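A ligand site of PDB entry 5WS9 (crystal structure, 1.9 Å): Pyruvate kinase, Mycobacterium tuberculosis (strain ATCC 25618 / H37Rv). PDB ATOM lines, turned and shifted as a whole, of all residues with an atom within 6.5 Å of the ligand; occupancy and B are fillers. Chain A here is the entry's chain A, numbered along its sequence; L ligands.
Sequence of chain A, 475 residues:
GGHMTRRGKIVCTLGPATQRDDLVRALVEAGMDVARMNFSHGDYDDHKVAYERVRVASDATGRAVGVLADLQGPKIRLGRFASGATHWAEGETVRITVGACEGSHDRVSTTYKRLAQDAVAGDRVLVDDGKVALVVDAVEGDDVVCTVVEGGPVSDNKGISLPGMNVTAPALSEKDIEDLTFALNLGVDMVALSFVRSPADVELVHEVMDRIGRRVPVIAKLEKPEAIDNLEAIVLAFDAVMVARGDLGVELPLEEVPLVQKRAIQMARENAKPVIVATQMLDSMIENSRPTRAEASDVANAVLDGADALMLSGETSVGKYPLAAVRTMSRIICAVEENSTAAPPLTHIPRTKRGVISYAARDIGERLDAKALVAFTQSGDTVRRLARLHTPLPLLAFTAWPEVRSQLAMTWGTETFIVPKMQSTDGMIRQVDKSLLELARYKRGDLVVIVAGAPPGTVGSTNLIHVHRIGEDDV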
ATOM      1  N   ARG A 354     -24.283  23.432 -11.479  1.00  0.00           N
ATOM      2  CA  ARG A 354     -25.142  22.348 -11.899  1.00  0.00           C
ATOM      3  C   ARG A 354     -26.552  22.459 -11.321  1.00  0.00           C
ATOM      4  O   ARG A 354     -27.540  22.102 -11.977  1.00  0.00           O
ATOM      5  CB  ARG A 354     -24.542  20.974 -11.567  1.00  0.00           C
ATOM      6  CG  ARG A 354     -23.497  20.531 -12.623  1.00  0.00           C
ATOM      7  CD  ARG A 354     -22.718  19.323 -12.165  1.00  0.00           C
ATOM      8  NE  ARG A 354     -21.881  19.638 -11.010  1.00  0.00           N
ATOM      9  CZ  ARG A 354     -21.017  18.786 -10.460  1.00  0.00           C
ATOM     10  NH1 ARG A 354     -20.824  17.594 -11.017  1.00  0.00           N
ATOM     11  NH2 ARG A 354     -20.295  19.159  -9.400  1.00  0.00           N
ATOM     12  N   PHE A 376     -27.300  15.355 -19.704  1.00  0.00           N
ATOM     13  CA  PHE A 376     -26.073  14.575 -19.851  1.00  0.00           C
ATOM     14  C   PHE A 376     -25.315  14.588 -18.540  1.00  0.00           C
ATOM     15  O   PHE A 376     -25.150  15.639 -17.905  1.00  0.00           O
ATOM     16  CB  PHE A 376     -25.219  15.097 -21.008  1.00  0.00           C
ATOM     17  CG  PHE A 376     -25.699  14.642 -22.349  1.00  0.00           C
ATOM     18  CD1 PHE A 376     -26.840  15.203 -22.942  1.00  0.00           C
ATOM     19  CD2 PHE A 376     -25.069  13.612 -22.998  1.00  0.00           C
ATOM     20  CE1 PHE A 376     -27.303  14.727 -24.158  1.00  0.00           C
ATOM     21  CE2 PHE A 376     -25.536  13.126 -24.200  1.00  0.00           C
ATOM     22  CZ  PHE A 376     -26.661  13.664 -24.761  1.00  0.00           C
ATOM     23  N   THR A 377     -24.867  13.414 -18.130  1.00  0.00           N
ATOM     24  CA  THR A 377     -24.200  13.263 -16.862  1.00  0.00           C
ATOM     25  C   THR A 377     -23.216  12.136 -16.888  1.00  0.00           C
ATOM     26  O   THR A 377     -23.502  11.022 -17.347  1.00  0.00           O
ATOM     27  CB  THR A 377     -25.187  13.097 -15.704  1.00  0.00           C
ATOM     28  OG1 THR A 377     -24.495  13.252 -14.439  1.00  0.00           O
ATOM     29  CG2 THR A 377     -25.907  11.760 -15.786  1.00  0.00           C
ATOM     30  N   GLN A 378     -22.030  12.463 -16.435  1.00  0.00           N
ATOM     31  CA  GLN A 378     -20.922  11.558 -16.383  1.00  0.00           C
ATOM     32  C   GLN A 378     -20.853  10.833 -15.027  1.00  0.00           C
ATOM     33  O   GLN A 378     -20.530   9.653 -14.962  1.00  0.00           O
ATOM     34  CB  GLN A 378     -19.647  12.376 -16.614  1.00  0.00           C
ATOM     35  CG  GLN A 378     -18.407  11.558 -16.672  1.00  0.00           C
ATOM     36  CD  GLN A 378     -17.329  12.258 -17.463  1.00  0.00           C
ATOM     37  OE1 GLN A 378     -17.628  13.044 -18.376  1.00  0.00           O
ATOM     38  NE2 GLN A 378     -16.071  11.965 -17.130  1.00  0.00           N
ATOM     39  N   SER A 379     -21.177  11.559 -13.946  1.00  0.00           N
ATOM     40  CA  SER A 379     -21.171  11.002 -12.577  1.00  0.00           C
ATOM     41  C   SER A 379     -22.562  10.777 -12.042  1.00  0.00           C
ATOM     42  O   SER A 379     -22.734  10.150 -10.987  1.00  0.00           O
ATOM     43  CB  SER A 379     -20.437  11.981 -11.629  1.00  0.00           C
ATOM     44  OG  SER A 379     -21.232  13.135 -11.374  1.00  0.00           O
ATOM     45  N   GLY A 380     -23.560  11.348 -12.711  1.00  0.00           N
ATOM     46  CA  GLY A 380     -24.935  11.364 -12.165  1.00  0.00           C
ATOM     47  C   GLY A 380     -25.360  12.686 -11.557  1.00  0.00           C
ATOM     48  O   GLY A 380     -26.522  12.957 -11.454  1.00  0.00           O
ATOM     49  N   ASP A 381     -24.394  13.524 -11.182  1.00  0.00           N
ATOM     50  CA  ASP A 381     -24.656  14.709 -10.388  1.00  0.00           C
ATOM     51  C   ASP A 381     -25.687  15.669 -11.026  1.00  0.00           C
ATOM     52  O   ASP A 381     -26.628  16.080 -10.376  1.00  0.00           O
ATOM     53  CB  ASP A 381     -23.351  15.476 -10.105  1.00  0.00           C
ATOM     54  CG  ASP A 381     -23.571  16.662  -9.198  1.00  0.00           C
ATOM     55  OD1 ASP A 381     -24.047  17.732  -9.676  1.00  0.00           O
ATOM     56  OD2 ASP A 381     -23.309  16.528  -7.991  1.00  0.00           O
ATOM     57  N   THR A 382     -25.516  15.996 -12.286  1.00  0.00           N
ATOM     58  CA  THR A 382     -26.383  16.994 -12.927  1.00  0.00           C
ATOM     59  C   THR A 382     -27.837  16.495 -12.890  1.00  0.00           C
ATOM     60  O   THR A 382     -28.758  17.277 -12.570  1.00  0.00           O
ATOM     61  CB  THR A 382     -25.938  17.294 -14.370  1.00  0.00           C
ATOM     62  OG1 THR A 382     -24.613  17.858 -14.359  1.00  0.00           O
ATOM     63  CG2 THR A 382     -26.878  18.265 -15.033  1.00  0.00           C
ATOM     64  N   VAL A 383     -28.014  15.203 -13.166  1.00  0.00           N
ATOM     65  CA  VAL A 383     -29.328  14.562 -13.143  1.00  0.00           C
ATOM     66  C   VAL A 383     -29.908  14.497 -11.726  1.00  0.00           C
ATOM     67  O   VAL A 383     -31.101  14.797 -11.512  1.00  0.00           O
ATOM     68  CB  VAL A 383     -29.251  13.141 -13.743  1.00  0.00           C
ATOM     69  CG1 VAL A 383     -30.500  12.325 -13.428  1.00  0.00           C
ATOM     70  CG2 VAL A 383     -29.064  13.217 -15.222  1.00  0.00           C
ATOM     71  N   PHE A 398     -28.627  10.953 -19.906  1.00  0.00           N
ATOM     72  CA  PHE A 398     -27.793  10.432 -20.984  1.00  0.00           C
ATOM     73  C   PHE A 398     -26.363  10.362 -20.484  1.00  0.00           C
ATOM     74  O   PHE A 398     -25.890  11.290 -19.817  1.00  0.00           O
ATOM     75  CB  PHE A 398     -27.875  11.324 -22.222  1.00  0.00           C
ATOM     76  CG  PHE A 398     -29.025  10.996 -23.132  1.00  0.00           C
ATOM     77  CD1 PHE A 398     -30.318  11.209 -22.732  1.00  0.00           C
ATOM     78  CD2 PHE A 398     -28.802  10.440 -24.361  1.00  0.00           C
ATOM     79  CE1 PHE A 398     -31.388  10.865 -23.561  1.00  0.00           C
ATOM     80  CE2 PHE A 398     -29.858  10.122 -25.188  1.00  0.00           C
ATOM     81  CZ  PHE A 398     -31.143  10.320 -24.790  1.00  0.00           C
ATOM     82  N   THR A 399     -25.699   9.233 -20.746  1.00  0.00           N
ATOM     83  CA  THR A 399     -24.368   9.036 -20.257  1.00  0.00           C
ATOM     84  C   THR A 399     -23.609   8.077 -21.209  1.00  0.00           C
ATOM     85  O   THR A 399     -24.223   7.362 -22.018  1.00  0.00           O
ATOM     86  CB  THR A 399     -24.401   8.426 -18.834  1.00  0.00           C
ATOM     87  OG1 THR A 399     -23.090   8.392 -18.269  1.00  0.00           O
ATOM     88  CG2 THR A 399     -24.943   6.990 -18.863  1.00  0.00           C
ATOM     89  N   ALA A 400     -22.287   8.052 -21.084  1.00  0.00           N
ATOM     90  CA  ALA A 400     -21.459   7.106 -21.817  1.00  0.00           C
ATOM     91  C   ALA A 400     -20.986   5.956 -20.935  1.00  0.00           C
ATOM     92  O   ALA A 400     -20.420   5.002 -21.424  1.00  0.00           O
ATOM     93  CB  ALA A 400     -20.259   7.838 -22.431  1.00  0.00           C
ATOM     94  N   TRP A 401     -21.263   6.046 -19.634  1.00  0.00           N
ATOM     95  CA  TRP A 401     -20.739   5.099 -18.661  1.00  0.00           C
ATOM     96  C   TRP A 401     -21.851   4.161 -18.172  1.00  0.00           C
ATOM     97  O   TRP A 401     -22.760   4.607 -17.470  1.00  0.00           O
ATOM     98  CB  TRP A 401     -20.081   5.851 -17.515  1.00  0.00           C
ATOM     99  CG  TRP A 401     -18.935   6.623 -18.001  1.00  0.00           C
ATOM    100  CD1 TRP A 401     -17.606   6.202 -18.055  1.00  0.00           C
ATOM    101  CD2 TRP A 401     -18.970   7.895 -18.658  1.00  0.00           C
ATOM    102  NE1 TRP A 401     -16.822   7.189 -18.647  1.00  0.00           N
ATOM    103  CE2 TRP A 401     -17.630   8.223 -19.030  1.00  0.00           C
ATOM    104  CE3 TRP A 401     -19.992   8.808 -18.947  1.00  0.00           C
ATOM    105  CZ2 TRP A 401     -17.307   9.428 -19.687  1.00  0.00           C
ATOM    106  CZ3 TRP A 401     -19.675  10.014 -19.582  1.00  0.00           C
ATOM    107  CH2 TRP A 401     -18.343  10.324 -19.941  1.00  0.00           C
ATOM    108  N   VAL A 419     -25.026   6.141 -24.448  1.00  0.00           N
ATOM    109  CA  VAL A 419     -24.670   6.559 -25.790  1.00  0.00           C
ATOM    110  C   VAL A 419     -23.153   6.664 -25.858  1.00  0.00           C
ATOM    111  O   VAL A 419     -22.475   6.563 -24.834  1.00  0.00           O
ATOM    112  CB  VAL A 419     -25.329   7.889 -26.167  1.00  0.00           C
ATOM    113  CG1 VAL A 419     -26.857   7.773 -26.157  1.00  0.00           C
ATOM    114  CG2 VAL A 419     -24.877   9.023 -25.257  1.00  0.00           C
ATOM    115  N   PRO A 420     -22.615   6.824 -27.064  1.00  0.00           N
ATOM    116  CA  PRO A 420     -21.175   6.971 -27.152  1.00  0.00           C
ATOM    117  C   PRO A 420     -20.642   8.205 -26.448  1.00  0.00           C
ATOM    118  O   PRO A 420     -21.366   9.155 -26.252  1.00  0.00           O
ATOM    119  CB  PRO A 420     -20.923   7.040 -28.671  1.00  0.00           C
ATOM    120  CG  PRO A 420     -22.082   6.338 -29.294  1.00  0.00           C
ATOM    121  CD  PRO A 420     -23.248   6.608 -28.380  1.00  0.00           C
ATOM    122  N   LYS A 421     -19.372   8.176 -26.086  1.00  0.00           N
ATOM    123  CA  LYS A 421     -18.694   9.373 -25.583  1.00  0.00           C
ATOM    124  C   LYS A 421     -18.487  10.346 -26.766  1.00  0.00           C
ATOM    125  O   LYS A 421     -17.879  10.007 -27.766  1.00  0.00           O
ATOM    126  CB  LYS A 421     -17.343   8.994 -24.965  1.00  0.00           C
ATOM    127  CG  LYS A 421     -16.756  10.106 -24.111  1.00  0.00           C
ATOM    128  CD  LYS A 421     -15.526   9.654 -23.353  1.00  0.00           C
ATOM    129  CE  LYS A 421     -14.858  10.867 -22.720  1.00  0.00           C
ATOM    130  NZ  LYS A 421     -13.385  10.690 -22.689  1.00  0.00           N
ATOM    131  N   MET A 422     -19.035  11.538 -26.644  1.00  0.00           N
ATOM    132  CA  MET A 422     -19.071  12.463 -27.752  1.00  0.00           C
ATOM    133  C   MET A 422     -18.059  13.542 -27.552  1.00  0.00           C
ATOM    134  O   MET A 422     -17.637  13.818 -26.420  1.00  0.00           O
ATOM    135  CB  MET A 422     -20.460  13.092 -27.879  1.00  0.00           C
ATOM    136  CG  MET A 422     -21.602  12.103 -27.922  1.00  0.00           C
ATOM    137  SD  MET A 422     -21.396  10.854 -29.198  1.00  0.00           S
ATOM    138  CE  MET A 422     -21.389  11.880 -30.674  1.00  0.00           C
ATOM    139  N   GLN A 423     -17.696  14.173 -28.657  1.00  0.00           N
ATOM    140  CA  GLN A 423     -16.638  15.169 -28.696  1.00  0.00           C
ATOM    141  C   GLN A 423     -17.162  16.593 -28.762  1.00  0.00           C
ATOM    142  O   GLN A 423     -16.397  17.510 -28.834  1.00  0.00           O
ATOM    143  CB  GLN A 423     -15.693  14.893 -29.872  1.00  0.00           C
ATOM    144  CG  GLN A 423     -14.819  13.671 -29.690  1.00  0.00           C
ATOM    145  CD  GLN A 423     -14.063  13.695 -28.371  1.00  0.00           C
ATOM    146  OE1 GLN A 423     -14.008  12.691 -27.643  1.00  0.00           O
ATOM    147  NE2 GLN A 423     -13.513  14.860 -28.023  1.00  0.00           N
ATOM    148  N   SER A 424     -18.480  16.749 -28.731  1.00  0.00           N
ATOM    149  CA  SER A 424     -19.089  18.062 -28.828  1.00  0.00           C
ATOM    150  C   SER A 424     -20.519  18.005 -28.288  1.00  0.00           C
ATOM    151  O   SER A 424     -21.137  16.942 -28.224  1.00  0.00           O
ATOM    152  CB  SER A 424     -19.124  18.507 -30.301  1.00  0.00           C
ATOM    153  OG  SER A 424     -20.117  17.770 -31.005  1.00  0.00           O
ATOM    154  N   THR A 425     -21.043  19.159 -27.872  1.00  0.00           N
ATOM    155  CA  THR A 425     -22.413  19.205 -27.437  1.00  0.00           C
ATOM    156  C   THR A 425     -23.388  19.011 -28.609  1.00  0.00           C
ATOM    157  O   THR A 425     -24.484  18.466 -28.421  1.00  0.00           O
ATOM    158  CB  THR A 425     -22.750  20.511 -26.662  1.00  0.00           C
ATOM    159  OG1 THR A 425     -22.504  21.648 -27.502  1.00  0.00           O
ATOM    160  CG2 THR A 425     -21.926  20.601 -25.339  1.00  0.00           C
ATOM    161  N   MET A 428     -23.724  15.370 -28.759  1.00  0.00           N
ATOM    162  CA  MET A 428     -24.635  14.967 -27.686  1.00  0.00           C
ATOM    163  C   MET A 428     -26.092  15.122 -28.090  1.00  0.00           C
ATOM    164  O   MET A 428     -26.901  14.208 -27.910  1.00  0.00           O
ATOM    165  CB  MET A 428     -24.344  15.744 -26.402  1.00  0.00           C
ATOM    166  CG  MET A 428     -22.986  15.441 -25.790  1.00  0.00           C
ATOM    167  SD  MET A 428     -22.699  16.466 -24.329  1.00  0.00           S
ATOM    168  CE  MET A 428     -20.918  16.736 -24.389  1.00  0.00           C
ATOM    169  N   GLN A 431     -27.223  12.574 -30.510  1.00  0.00           N
ATOM    170  CA  GLN A 431     -27.424  11.281 -29.846  1.00  0.00           C
ATOM    171  C   GLN A 431     -28.780  11.227 -29.145  1.00  0.00           C
ATOM    172  O   GLN A 431     -29.413  10.148 -29.061  1.00  0.00           O
ATOM    173  CB  GLN A 431     -26.275  10.954 -28.865  1.00  0.00           C
ATOM    174  CG  GLN A 431     -24.945  10.634 -29.556  1.00  0.00           C
ATOM    175  CD  GLN A 431     -25.016   9.359 -30.397  1.00  0.00           C
ATOM    176  OE1 GLN A 431     -25.710   8.403 -30.047  1.00  0.00           O
ATOM    177  NE2 GLN A 431     -24.308   9.351 -31.507  1.00  0.00           N
ATOM    178  N   VAL A 451     -29.930  19.584 -21.257  1.00  0.00           N
ATOM    179  CA  VAL A 451     -28.857  20.123 -20.463  1.00  0.00           C
ATOM    180  C   VAL A 451     -27.568  19.372 -20.794  1.00  0.00           C
ATOM    181  O   VAL A 451     -27.546  18.130 -20.774  1.00  0.00           O
ATOM    182  CB  VAL A 451     -29.135  19.981 -18.980  1.00  0.00           C
ATOM    183  CG1 VAL A 451     -27.942  20.455 -18.177  1.00  0.00           C
ATOM    184  CG2 VAL A 451     -30.347  20.776 -18.591  1.00  0.00           C
ATOM    185  N   ALA A 452     -26.505  20.103 -21.082  1.00  0.00           N
ATOM    186  CA  ALA A 452     -25.237  19.504 -21.467  1.00  0.00           C
ATOM    187  C   ALA A 452     -24.096  20.431 -21.103  1.00  0.00           C
ATOM    188  O   ALA A 452     -24.309  21.498 -20.559  1.00  0.00           O
ATOM    189  CB  ALA A 452     -25.209  19.190 -22.968  1.00  0.00           C
ATOM    190  N   GLY A 453     -22.864  20.038 -21.399  1.00  0.00           N
ATOM    191  CA  GLY A 453     -21.747  20.867 -21.074  1.00  0.00           C
ATOM    192  C   GLY A 453     -20.479  20.554 -21.854  1.00  0.00           C
ATOM    193  O   GLY A 453     -20.209  19.402 -22.168  1.00  0.00           O
ATOM    194  N   ALA A 454     -19.695  21.600 -22.098  1.00  0.00           N
ATOM    195  CA  ALA A 454     -18.346  21.480 -22.590  1.00  0.00           C
ATOM    196  C   ALA A 454     -17.390  22.118 -21.567  1.00  0.00           C
ATOM    197  O   ALA A 454     -17.775  23.096 -20.905  1.00  0.00           O
ATOM    198  CB  ALA A 454     -18.217  22.169 -23.950  1.00  0.00           C
ATOM    199  N   PRO A 455     -16.166  21.589 -21.444  1.00  0.00           N
ATOM    200  CA  PRO A 455     -15.624  20.562 -22.374  1.00  0.00           C
ATOM    201  C   PRO A 455     -16.312  19.209 -22.203  1.00  0.00           C
ATOM    202  O   PRO A 455     -16.657  18.804 -21.067  1.00  0.00           O
ATOM    203  CB  PRO A 455     -14.128  20.458 -22.008  1.00  0.00           C
ATOM    204  CG  PRO A 455     -13.912  21.341 -20.831  1.00  0.00           C
ATOM    205  CD  PRO A 455     -15.149  22.173 -20.565  1.00  0.00           C
ATOM    206  N   PRO A 456     -16.538  18.496 -23.326  1.00  0.00           N
ATOM    207  CA  PRO A 456     -17.245  17.221 -23.274  1.00  0.00           C
ATOM    208  C   PRO A 456     -16.485  16.237 -22.407  1.00  0.00           C
ATOM    209  O   PRO A 456     -15.272  16.393 -22.244  1.00  0.00           O
ATOM    210  CB  PRO A 456     -17.218  16.744 -24.736  1.00  0.00           C
ATOM    211  CG  PRO A 456     -16.953  17.960 -25.546  1.00  0.00           C
ATOM    212  CD  PRO A 456     -16.090  18.833 -24.687  1.00  0.00           C
ATOM    213  N   GLY A 457     -17.184  15.274 -21.823  1.00  0.00           N
ATOM    214  CA  GLY A 457     -16.486  14.192 -21.142  1.00  0.00           C
ATOM    215  C   GLY A 457     -15.757  14.636 -19.904  1.00  0.00           C
ATOM    216  O   GLY A 457     -14.839  13.971 -19.478  1.00  0.00           O
ATOM    217  N   THR A 458     -16.198  15.727 -19.284  1.00  0.00           N
ATOM    218  CA  THR A 458     -15.613  16.251 -18.068  1.00  0.00           C
ATOM    219  C   THR A 458     -16.704  16.419 -16.983  1.00  0.00           C
ATOM    220  O   THR A 458     -17.693  17.136 -17.180  1.00  0.00           O
ATOM    221  CB  THR A 458     -14.982  17.611 -18.364  1.00  0.00           C
ATOM    222  OG1 THR A 458     -14.077  17.477 -19.488  1.00  0.00           O
ATOM    223  CG2 THR A 458     -14.229  18.190 -17.112  1.00  0.00           C
ATOM    224  N   VAL A 459     -16.512  15.783 -15.835  1.00  0.00           N
ATOM    225  CA  VAL A 459     -17.463  15.957 -14.748  1.00  0.00           C
ATOM    226  C   VAL A 459     -17.558  17.431 -14.377  1.00  0.00           C
ATOM    227  O   VAL A 459     -16.533  18.123 -14.262  1.00  0.00           O
ATOM    228  CB  VAL A 459     -17.103  15.118 -13.493  1.00  0.00           C
ATOM    229  CG1 VAL A 459     -17.948  15.530 -12.270  1.00  0.00           C
ATOM    230  CG2 VAL A 459     -17.321  13.645 -13.781  1.00  0.00           C
ATOM    231  N   GLY A 460     -18.785  17.929 -14.269  1.00  0.00           N
ATOM    232  CA  GLY A 460     -19.023  19.275 -13.771  1.00  0.00           C
ATOM    233  C   GLY A 460     -19.083  20.345 -14.827  1.00  0.00           C
ATOM    234  O   GLY A 460     -19.287  21.529 -14.512  1.00  0.00           O
ATOM    235  N   SER A 461     -18.879  19.972 -16.092  1.00  0.00           N
ATOM    236  CA  SER A 461     -18.729  21.008 -17.131  1.00  0.00           C
ATOM    237  C   SER A 461     -20.077  21.573 -17.559  1.00  0.00           C
ATOM    238  O   SER A 461     -20.124  22.571 -18.267  1.00  0.00           O
ATOM    239  CB  SER A 461     -17.943  20.468 -18.345  1.00  0.00           C
ATOM    240  OG  SER A 461     -18.672  19.450 -19.026  1.00  0.00           O
ATOM    241  N   THR A 462     -21.170  20.925 -17.125  1.00  0.00           N
ATOM    242  CA  THR A 462     -22.546  21.379 -17.407  1.00  0.00           C
ATOM    243  C   THR A 462     -22.648  22.910 -17.507  1.00  0.00           C
ATOM    244  O   THR A 462     -22.389  23.651 -16.525  1.00  0.00           O
ATOM    245  CB  THR A 462     -23.485  20.820 -16.343  1.00  0.00           C
ATOM    246  OG1 THR A 462     -23.426  19.380 -16.360  1.00  0.00           O
ATOM    247  CG2 THR A 462     -24.926  21.248 -16.576  1.00  0.00           C
ATOM    248  N   ASN A 463     -22.968  23.404 -18.708  1.00  0.00           N
ATOM    249  CA  ASN A 463     -22.996  24.837 -18.928  1.00  0.00           C
ATOM    250  C   ASN A 463     -23.915  25.336 -20.034  1.00  0.00           C
ATOM    251  O   ASN A 463     -23.855  26.509 -20.414  1.00  0.00           O
ATOM    252  CB  ASN A 463     -21.594  25.398 -19.091  1.00  0.00           C
ATOM    253  CG  ASN A 463     -20.930  24.978 -20.401  1.00  0.00           C
ATOM    254  OD1 ASN A 463     -21.385  24.042 -21.091  1.00  0.00           O
ATOM    255  ND2 ASN A 463     -19.834  25.626 -20.728  1.00  0.00           N
HETATM  256  P1  LIG L   1     -21.834  15.533 -14.264  1.00  0.00           P
HETATM  257  O1  LIG L   1     -21.160  14.363 -13.599  1.00  0.00           O
HETATM  258  O2  LIG L   1     -23.349  15.460 -14.178  1.00  0.00           O
HETATM  259  O3  LIG L   1     -21.265  16.807 -13.727  1.00  0.00           O
HETATM  260  O4  LIG L   1     -21.498  15.390 -15.830  1.00  0.00           O
HETATM  261  C1  LIG L   1     -22.021  16.322 -16.783  1.00  0.00           C
HETATM  262  C2  LIG L   1     -21.098  16.256 -18.007  1.00  0.00           C
HETATM  263  O5  LIG L   1     -20.952  14.909 -18.458  1.00  0.00           O
HETATM  264  C3  LIG L   1     -21.573  17.047 -19.191  1.00  0.00           C
HETATM  265  O6  LIG L   1     -21.097  18.393 -19.027  1.00  0.00           O
HETATM  266  C4  LIG L   1     -20.913  16.320 -20.363  1.00  0.00           C
HETATM  267  O7  LIG L   1     -19.734  17.041 -20.728  1.00  0.00           O
HETATM  268  C5  LIG L   1     -20.513  14.953 -19.809  1.00  0.00           C
HETATM  269  N1  LIG L   1     -21.134  13.852 -20.574  1.00  0.00           N
HETATM  270  C6  LIG L   1     -22.151  13.053 -20.188  1.00  0.00           C
HETATM  271  N2  LIG L   1     -22.464  12.147 -21.158  1.00  0.00           N
HETATM  272  C7  LIG L   1     -21.574  12.327 -22.147  1.00  0.00           C
HETATM  273  C8  LIG L   1     -21.316  11.712 -23.448  1.00  0.00           C
HETATM  274  N3  LIG L   1     -22.081  10.696 -23.921  1.00  0.00           N
HETATM  275  N4  LIG L   1     -20.307  12.239 -24.184  1.00  0.00           N
HETATM  276  C9  LIG L   1     -19.561  13.258 -23.753  1.00  0.00           C
HETATM  277  N5  LIG L   1     -19.739  13.863 -22.570  1.00  0.00           N
HETATM  278  C10 LIG L   1     -20.714  13.447 -21.752  1.00  0.00           C
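Phe 376 touches the ligand. N of Gly 380 touches O1 of the ligand, 3.95 Å away. Asp 381 touches the ligand. Phe 398 touches the ligand (O to N2, 3.8 Å). CA of Thr 399 touches N2 of the ligand (3.8 Å). Ala 400 touches the ligand. CZ3 of Trp 401 touches N2 of the ligand, at 3.8 Å. Val 419 touches the ligand. Lys 421 touches the ligand (CA to N4, 3.6 Å). CE of Met 428 touches N5 of the ligand (3.6 Å). O of Pro 455 touches O7 of the ligand (3.6 Å). Pro 456 touches the ligand. Thr 458 touches the ligand (O to C2, 3.6 Å). CG1 of Val 459 touches O1 of the ligand (3.7 Å). Hydrophobic or aromatic side chains within 4 Å of the ligand: Phe 376, Ala 400, Trp 401, Val 419, Met 422, Met 428 and Val 459.
The side-chain hydroxyl of Thr 377 is in hydrogen-bond range of the backbone NH of Asp 381 (3.3 Å). O of Thr 377 lies within hydrogen-bond range of OG1 of Thr 399 (2.8 Å). The backbone NH (N) of Thr 377 lies within hydrogen-bond range of the backbone carbonyl oxygen (O) of Phe 398. The side-chain hydroxyl (OG1) of Thr 377 sits at hydrogen-bond distance from the backbone NH (N) of Gly 380. The side-chain hydroxyl (OG) of Ser 379 sits at hydrogen-bond distance from the backbone NH (N) of Asp 381. The side-chain hydroxyl (OG1) of Thr 462 lies within hydrogen-bond range of the side-chain hydroxyl (OG1) of Thr 382 (2.8 Å). N of Phe 376 is in hydrogen-bond range of O of Val 451. N of Val 419 sits at hydrogen-bond distance from O of Thr 399.
O2 of the ligand lies within hydrogen-bond range of OG1 of Thr 377, 2.5 Å away. An oxygen (O1) of the ligand lies within hydrogen-bond range of the backbone NH (N) of Ser 379. O1 of the ligand sits at hydrogen-bond distance from OG of Ser 379, at 2.5 Å. O6 of the ligand sits at hydrogen-bond distance from OG of Ser 461 (2.6 Å). N of Thr 382 lies within hydrogen-bond range of O2 of the ligand (2.9 Å). The side-chain hydroxyl (OG1) of Thr 382 lies within hydrogen-bond range of an oxygen (O2) of the ligand, at 2.7 Å. The backbone NH (N) of Gly 460 sits at hydrogen-bond distance from an oxygen (O3) of the ligand (2.8 Å). N of Gly 453 lies close to O6 of the ligand (3.4 Å). The backbone carbonyl oxygen of Gly 453 lies within hydrogen-bond range of an oxygen (O7) of the ligand (2.8 Å). An oxygen (O3) of the ligand lies within salt-bridge range of the guanidinium group of Arg 354 (2.9 Å). A nitrogen (N4) of the ligand is in hydrogen-bond range of the backbone NH of Met 422 (2.9 Å). O of Pro 420 sits at hydrogen-bond distance from N3 of the ligand, at 2.9 Å. A nitrogen (N5) of the ligand lies within hydrogen-bond range of the backbone NH of Gly 457. N of Gln 378 lies within hydrogen-bond range of O4 of the ligand, at 3.0 Å. The backbone NH of Thr 462 lies within hydrogen-bond range of an oxygen (O6) of the ligand.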
